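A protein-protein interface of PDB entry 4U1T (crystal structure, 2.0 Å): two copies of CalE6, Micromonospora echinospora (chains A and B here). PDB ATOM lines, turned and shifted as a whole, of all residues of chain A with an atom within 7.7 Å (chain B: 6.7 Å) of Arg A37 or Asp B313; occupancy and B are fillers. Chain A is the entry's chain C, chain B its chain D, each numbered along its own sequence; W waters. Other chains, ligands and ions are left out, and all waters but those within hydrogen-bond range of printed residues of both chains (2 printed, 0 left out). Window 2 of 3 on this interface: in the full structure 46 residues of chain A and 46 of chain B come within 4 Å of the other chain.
Of the printed residues of chain B, Glu A35 touches Thr B319 (3.3 Å) and Cys B320 (3.2 Å). Printed residues of chain B within 4 Å of Arg A36: Cys B320 (2.9 Å). Arg A37 touches five residues of chain B. Printed residues of chain A within 4 Å of Leu B312: Arg A37 (2.8 Å). Of chain A, only Arg A37 (3.5 Å) comes within 4 Å of Asp B313. Of the printed residues of chain A, Thr B319 touches Glu A35. Of the printed residues of chain A, Cys B320 touches Tyr A34 (3.7 Å), Glu A35 (3.2 Å), Arg A36 (2.9 Å) and Arg A37 (3.6 Å). The nearest residue of chain B that does not touch Arg A37 is Arg B314 (4.2 Å).
Water W2 lies within hydrogen-bond range of the backbone carbonyl oxygen (O) of Phe B318, the guanidinium group (NH2) of Arg A37, the backbone carbonyl oxygen (O) of Phe B315 and the backbone NH (N) of Leu B317. Water W1 bridges the side-chain hydroxyl (OG1) of Thr B319 (2.8 Å) and the side-chain carboxylate (OE1) of Glu A35 (3.0 Å).
No position is printed for both chains.
O of Cys B320 touches O of Tyr A34 (3.7 Å). Thr B319 touches Glu A35. Asp B313 touches Arg A37. Phe B318 touches Arg A37. NE of Arg A37 touches CB of Cys B320, at 3.6 Å.
OE1 of Glu A35 is in hydrogen-bond range of N of Cys B320. The backbone NH of Arg A36 sits at hydrogen-bond distance from the backbone carbonyl oxygen of Cys B320 (2.9 Å). The backbone carbonyl oxygen (O) of Leu B312 sits at hydrogen-bond distance from the guanidinium group (NH1) of Arg A37 (2.8 Å). The guanidinium group (NH1) of Arg A37 is in hydrogen-bond range of the backbone carbonyl oxygen (O) of Phe B315 (2.9 Å).
OE2 of Glu A35 is in salt-bridge range of NE of Arg A37, 2.8 Å away. The backbone carbonyl oxygen (O) of Glu A35 is in hydrogen-bond range of the side-chain amide nitrogen (NE2) of Gln A39, 3.3 Å away. The backbone NH of Val B331 is in hydrogen-bond range of the backbone carbonyl oxygen of Thr B319 (2.9 Å).
Of the 6 printed residues of chain A, 4 touch a printed residue of chain B. Among the printed residues, no Asp or Glu carboxylate lies within 4 Å of a Lys or Arg side-chain nitrogen of the other chain.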
ATOM      1  N   TYR A  34      10.724 -28.229 -31.301  1.00  0.00           N
ATOM      2  CA  TYR A  34       9.588 -29.130 -31.392  1.00  0.00           C
ATOM      3  C   TYR A  34       8.457 -28.640 -30.525  1.00  0.00           C
ATOM      4  O   TYR A  34       8.691 -28.152 -29.415  1.00  0.00           O
ATOM      5  CB  TYR A  34       9.986 -30.526 -30.947  1.00  0.00           C
ATOM      6  CG  TYR A  34      11.131 -31.098 -31.720  1.00  0.00           C
ATOM      7  CD1 TYR A  34      12.439 -30.928 -31.276  1.00  0.00           C
ATOM      8  CD2 TYR A  34      10.920 -31.793 -32.901  1.00  0.00           C
ATOM      9  CE1 TYR A  34      13.496 -31.443 -31.974  1.00  0.00           C
ATOM     10  CE2 TYR A  34      11.971 -32.311 -33.606  1.00  0.00           C
ATOM     11  CZ  TYR A  34      13.262 -32.140 -33.134  1.00  0.00           C
ATOM     12  OH  TYR A  34      14.333 -32.658 -33.827  1.00  0.00           O
ATOM     13  N   GLU A  35       7.235 -28.794 -31.024  1.00  0.00           N
ATOM     14  CA  GLU A  35       6.045 -28.426 -30.277  1.00  0.00           C
ATOM     15  C   GLU A  35       5.811 -29.520 -29.245  1.00  0.00           C
ATOM     16  O   GLU A  35       5.734 -30.707 -29.588  1.00  0.00           O
ATOM     17  CB  GLU A  35       4.844 -28.245 -31.230  1.00  0.00           C
ATOM     18  CG  GLU A  35       3.454 -28.300 -30.574  1.00  0.00           C
ATOM     19  CD  GLU A  35       3.130 -27.108 -29.674  1.00  0.00           C
ATOM     20  OE1 GLU A  35       2.996 -25.975 -30.194  1.00  0.00           O
ATOM     21  OE2 GLU A  35       2.979 -27.309 -28.449  1.00  0.00           O
ATOM     22  N   ARG A  36       5.734 -29.114 -27.980  1.00  0.00           N
ATOM     23  CA  ARG A  36       5.639 -30.055 -26.873  1.00  0.00           C
ATOM     24  C   ARG A  36       4.251 -30.695 -26.807  1.00  0.00           C
ATOM     25  O   ARG A  36       4.127 -31.878 -26.489  1.00  0.00           O
ATOM     26  CB  ARG A  36       5.981 -29.358 -25.551  1.00  0.00           C
ATOM     27  N   ARG A  37       3.213 -29.920 -27.114  1.00  0.00           N
ATOM     28  CA  ARG A  37       1.836 -30.417 -27.029  1.00  0.00           C
ATOM     29  C   ARG A  37       1.464 -31.348 -28.195  1.00  0.00           C
ATOM     30  O   ARG A  37       0.370 -31.911 -28.223  1.00  0.00           O
ATOM     31  CB  ARG A  37       0.848 -29.243 -26.959  1.00  0.00           C
ATOM     32  CG  ARG A  37       1.089 -28.281 -25.797  1.00  0.00           C
ATOM     33  CD  ARG A  37       0.319 -26.973 -25.975  1.00  0.00           C
ATOM     34  NE  ARG A  37       0.753 -26.274 -27.179  1.00  0.00           N
ATOM     35  CZ  ARG A  37       0.181 -25.184 -27.679  1.00  0.00           C
ATOM     36  NH1 ARG A  37      -0.865 -24.635 -27.076  1.00  0.00           N
ATOM     37  NH2 ARG A  37       0.671 -24.638 -28.790  1.00  0.00           N
ATOM     38  N   ALA A  38       2.371 -31.504 -29.154  1.00  0.00           N
ATOM     39  CA  ALA A  38       2.105 -32.306 -30.348  1.00  0.00           C
ATOM     40  C   ALA A  38       2.703 -33.708 -30.254  1.00  0.00           C
ATOM     41  O   ALA A  38       2.846 -34.396 -31.268  1.00  0.00           O
ATOM     42  CB  ALA A  38       2.634 -31.600 -31.590  1.00  0.00           C
ATOM     43  N   GLN A  39       3.066 -34.130 -29.047  1.00  0.00           N
ATOM     44  CA  GLN A  39       3.763 -35.401 -28.889  1.00  0.00           C
ATOM     45  C   GLN A  39       3.060 -36.338 -27.913  1.00  0.00           C
ATOM     46  O   GLN A  39       3.013 -37.545 -28.141  1.00  0.00           O
ATOM     47  CB  GLN A  39       5.206 -35.166 -28.432  1.00  0.00           C
ATOM     48  CG  GLN A  39       6.029 -34.299 -29.373  1.00  0.00           C
ATOM     49  CD  GLN A  39       7.485 -34.194 -28.944  1.00  0.00           C
ATOM     50  OE1 GLN A  39       8.154 -35.207 -28.717  1.00  0.00           O
ATOM     51  NE2 GLN A  39       7.986 -32.968 -28.845  1.00  0.00           N
ATOM     52  N   ALA B 308       0.923 -23.497 -14.976  1.00  0.00           N
ATOM     53  CA  ALA B 308       1.489 -23.002 -16.230  1.00  0.00           C
ATOM     54  C   ALA B 308       1.028 -23.830 -17.429  1.00  0.00           C
ATOM     55  O   ALA B 308       0.821 -23.280 -18.509  1.00  0.00           O
ATOM     56  CB  ALA B 308       3.008 -22.984 -16.155  1.00  0.00           C
ATOM     57  N   GLU B 309       0.864 -25.139 -17.234  1.00  0.00           N
ATOM     58  CA  GLU B 309       0.440 -26.047 -18.309  1.00  0.00           C
ATOM     59  C   GLU B 309      -0.910 -25.633 -18.867  1.00  0.00           C
ATOM     60  O   GLU B 309      -1.187 -25.808 -20.050  1.00  0.00           O
ATOM     61  CB  GLU B 309       0.324 -27.501 -17.833  1.00  0.00           C
ATOM     62  CG  GLU B 309       1.481 -28.049 -17.033  1.00  0.00           C
ATOM     63  CD  GLU B 309       1.316 -27.784 -15.552  1.00  0.00           C
ATOM     64  OE1 GLU B 309       1.278 -28.759 -14.767  1.00  0.00           O
ATOM     65  OE2 GLU B 309       1.212 -26.599 -15.175  1.00  0.00           O
ATOM     66  N   ARG B 310      -1.761 -25.105 -17.999  1.00  0.00           N
ATOM     67  CA  ARG B 310      -3.087 -24.680 -18.409  1.00  0.00           C
ATOM     68  C   ARG B 310      -2.989 -23.484 -19.343  1.00  0.00           C
ATOM     69  O   ARG B 310      -3.708 -23.402 -20.338  1.00  0.00           O
ATOM     70  CB  ARG B 310      -3.940 -24.342 -17.187  1.00  0.00           C
ATOM     71  CG  ARG B 310      -5.344 -23.863 -17.516  1.00  0.00           C
ATOM     72  N   LEU B 311      -2.107 -22.548 -19.016  1.00  0.00           N
ATOM     73  CA  LEU B 311      -1.893 -21.401 -19.885  1.00  0.00           C
ATOM     74  C   LEU B 311      -1.292 -21.856 -21.214  1.00  0.00           C
ATOM     75  O   LEU B 311      -1.798 -21.516 -22.283  1.00  0.00           O
ATOM     76  CB  LEU B 311      -0.988 -20.372 -19.206  1.00  0.00           C
ATOM     77  CG  LEU B 311      -0.635 -19.162 -20.068  1.00  0.00           C
ATOM     78  CD1 LEU B 311      -1.869 -18.290 -20.292  1.00  0.00           C
ATOM     79  CD2 LEU B 311       0.484 -18.371 -19.418  1.00  0.00           C
ATOM     80  N   LEU B 312      -0.240 -22.666 -21.139  1.00  0.00           N
ATOM     81  CA  LEU B 312       0.470 -23.122 -22.334  1.00  0.00           C
ATOM     82  C   LEU B 312      -0.449 -23.839 -23.331  1.00  0.00           C
ATOM     83  O   LEU B 312      -0.302 -23.681 -24.539  1.00  0.00           O
ATOM     84  CB  LEU B 312       1.630 -24.046 -21.933  1.00  0.00           C
ATOM     85  CG  LEU B 312       2.732 -23.396 -21.087  1.00  0.00           C
ATOM     86  CD1 LEU B 312       3.731 -24.425 -20.579  1.00  0.00           C
ATOM     87  CD2 LEU B 312       3.435 -22.332 -21.891  1.00  0.00           C
ATOM     88  N   ASP B 313      -1.401 -24.613 -22.816  1.00  0.00           N
ATOM     89  CA  ASP B 313      -2.332 -25.381 -23.646  1.00  0.00           C
ATOM     90  C   ASP B 313      -3.320 -24.535 -24.441  1.00  0.00           C
ATOM     91  O   ASP B 313      -3.929 -25.017 -25.399  1.00  0.00           O
ATOM     92  CB  ASP B 313      -3.132 -26.350 -22.769  1.00  0.00           C
ATOM     93  CG  ASP B 313      -2.326 -27.557 -22.338  1.00  0.00           C
ATOM     94  OD1 ASP B 313      -1.276 -27.831 -22.959  1.00  0.00           O
ATOM     95  OD2 ASP B 313      -2.753 -28.234 -21.378  1.00  0.00           O
ATOM     96  N   ARG B 314      -3.484 -23.282 -24.031  1.00  0.00           N
ATOM     97  CA  ARG B 314      -4.507 -22.404 -24.591  1.00  0.00           C
ATOM     98  C   ARG B 314      -4.014 -21.585 -25.789  1.00  0.00           C
ATOM     99  O   ARG B 314      -4.826 -21.025 -26.523  1.00  0.00           O
ATOM    100  CB  ARG B 314      -5.026 -21.472 -23.490  1.00  0.00           C
ATOM    101  CG  ARG B 314      -5.790 -22.208 -22.373  1.00  0.00           C
ATOM    102  CD  ARG B 314      -6.438 -21.257 -21.366  1.00  0.00           C
ATOM    103  NE  ARG B 314      -7.238 -20.218 -22.009  1.00  0.00           N
ATOM    104  CZ  ARG B 314      -8.527 -20.343 -22.313  1.00  0.00           C
ATOM    105  NH1 ARG B 314      -9.172 -21.469 -22.038  1.00  0.00           N
ATOM    106  NH2 ARG B 314      -9.171 -19.341 -22.895  1.00  0.00           N
ATOM    107  N   PHE B 315      -2.695 -21.507 -25.990  1.00  0.00           N
ATOM    108  CA  PHE B 315      -2.157 -20.767 -27.142  1.00  0.00           C
ATOM    109  C   PHE B 315      -2.489 -21.468 -28.455  1.00  0.00           C
ATOM    110  O   PHE B 315      -2.365 -22.687 -28.559  1.00  0.00           O
ATOM    111  CB  PHE B 315      -0.637 -20.587 -27.037  1.00  0.00           C
ATOM    112  CG  PHE B 315      -0.206 -19.623 -25.973  1.00  0.00           C
ATOM    113  CD1 PHE B 315      -0.173 -18.258 -26.230  1.00  0.00           C
ATOM    114  CD2 PHE B 315       0.188 -20.077 -24.729  1.00  0.00           C
ATOM    115  CE1 PHE B 315       0.240 -17.367 -25.261  1.00  0.00           C
ATOM    116  CE2 PHE B 315       0.592 -19.188 -23.745  1.00  0.00           C
ATOM    117  CZ  PHE B 315       0.616 -17.830 -24.012  1.00  0.00           C
ATOM    118  N   THR B 316      -2.877 -20.702 -29.469  1.00  0.00           N
ATOM    119  CA  THR B 316      -3.159 -21.293 -30.771  1.00  0.00           C
ATOM    120  C   THR B 316      -2.243 -20.749 -31.866  1.00  0.00           C
ATOM    121  O   THR B 316      -2.292 -21.216 -33.005  1.00  0.00           O
ATOM    122  CB  THR B 316      -4.625 -21.053 -31.200  1.00  0.00           C
ATOM    123  OG1 THR B 316      -4.879 -19.646 -31.237  1.00  0.00           O
ATOM    124  CG2 THR B 316      -5.595 -21.710 -30.217  1.00  0.00           C
ATOM    125  N   LEU B 317      -1.414 -19.764 -31.528  1.00  0.00           N
ATOM    126  CA  LEU B 317      -0.471 -19.211 -32.500  1.00  0.00           C
ATOM    127  C   LEU B 317       0.977 -19.337 -32.006  1.00  0.00           C
ATOM    128  O   LEU B 317       1.834 -19.846 -32.729  1.00  0.00           O
ATOM    129  CB  LEU B 317      -0.814 -17.750 -32.811  1.00  0.00           C
ATOM    130  CG  LEU B 317       0.066 -17.078 -33.872  1.00  0.00           C
ATOM    131  CD1 LEU B 317       0.124 -17.920 -35.135  1.00  0.00           C
ATOM    132  CD2 LEU B 317      -0.475 -15.690 -34.191  1.00  0.00           C
ATOM    133  N   PHE B 318       1.248 -18.863 -30.790  1.00  0.00           N
ATOM    134  CA  PHE B 318       2.501 -19.178 -30.112  1.00  0.00           C
ATOM    135  C   PHE B 318       2.668 -20.693 -30.095  1.00  0.00           C
ATOM    136  O   PHE B 318       1.700 -21.430 -29.904  1.00  0.00           O
ATOM    137  CB  PHE B 318       2.520 -18.656 -28.662  1.00  0.00           C
ATOM    138  CG  PHE B 318       2.769 -17.171 -28.532  1.00  0.00           C
ATOM    139  CD1 PHE B 318       1.726 -16.262 -28.663  1.00  0.00           C
ATOM    140  CD2 PHE B 318       4.040 -16.697 -28.237  1.00  0.00           C
ATOM    141  CE1 PHE B 318       1.951 -14.895 -28.525  1.00  0.00           C
ATOM    142  CE2 PHE B 318       4.274 -15.336 -28.100  1.00  0.00           C
ATOM    143  CZ  PHE B 318       3.229 -14.436 -28.244  1.00  0.00           C
ATOM    144  N   THR B 319       3.886 -21.145 -30.322  1.00  0.00           N
ATOM    145  CA  THR B 319       4.231 -22.557 -30.207  1.00  0.00           C
ATOM    146  C   THR B 319       4.859 -22.850 -28.862  1.00  0.00           C
ATOM    147  O   THR B 319       5.792 -22.156 -28.449  1.00  0.00           O
ATOM    148  CB  THR B 319       5.208 -22.964 -31.321  1.00  0.00           C
ATOM    149  OG1 THR B 319       4.527 -22.873 -32.571  1.00  0.00           O
ATOM    150  CG2 THR B 319       5.725 -24.395 -31.109  1.00  0.00           C
ATOM    151  N   CYS B 320       4.384 -23.897 -28.194  1.00  0.00           N
ATOM    152  CA  CYS B 320       4.975 -24.280 -26.926  1.00  0.00           C
ATOM    153  C   CYS B 320       6.215 -25.128 -27.174  1.00  0.00           C
ATOM    154  O   CYS B 320       6.122 -26.294 -27.546  1.00  0.00           O
ATOM    155  CB  CYS B 320       3.974 -25.034 -26.050  1.00  0.00           C
ATOM    156  SG  CYS B 320       4.691 -25.444 -24.428  1.00  0.00           S
ATOM    157  N   VAL B 331       6.610 -19.983 -26.773  1.00  0.00           N
ATOM    158  CA  VAL B 331       6.326 -19.777 -25.358  1.00  0.00           C
ATOM    159  C   VAL B 331       6.794 -21.007 -24.596  1.00  0.00           C
ATOM    160  O   VAL B 331       6.672 -22.135 -25.082  1.00  0.00           O
ATOM    161  CB  VAL B 331       4.817 -19.512 -25.102  1.00  0.00           C
ATOM    162  CG1 VAL B 331       3.963 -20.642 -25.668  1.00  0.00           C
ATOM    163  CG2 VAL B 331       4.531 -19.320 -23.599  1.00  0.00           C
HETATM  164  O   HOH W   1       2.654 -24.903 -32.994  1.00  0.00           O
HETATM  165  O   HOH W   2      -0.130 -22.897 -30.724  1.00  0.00           O
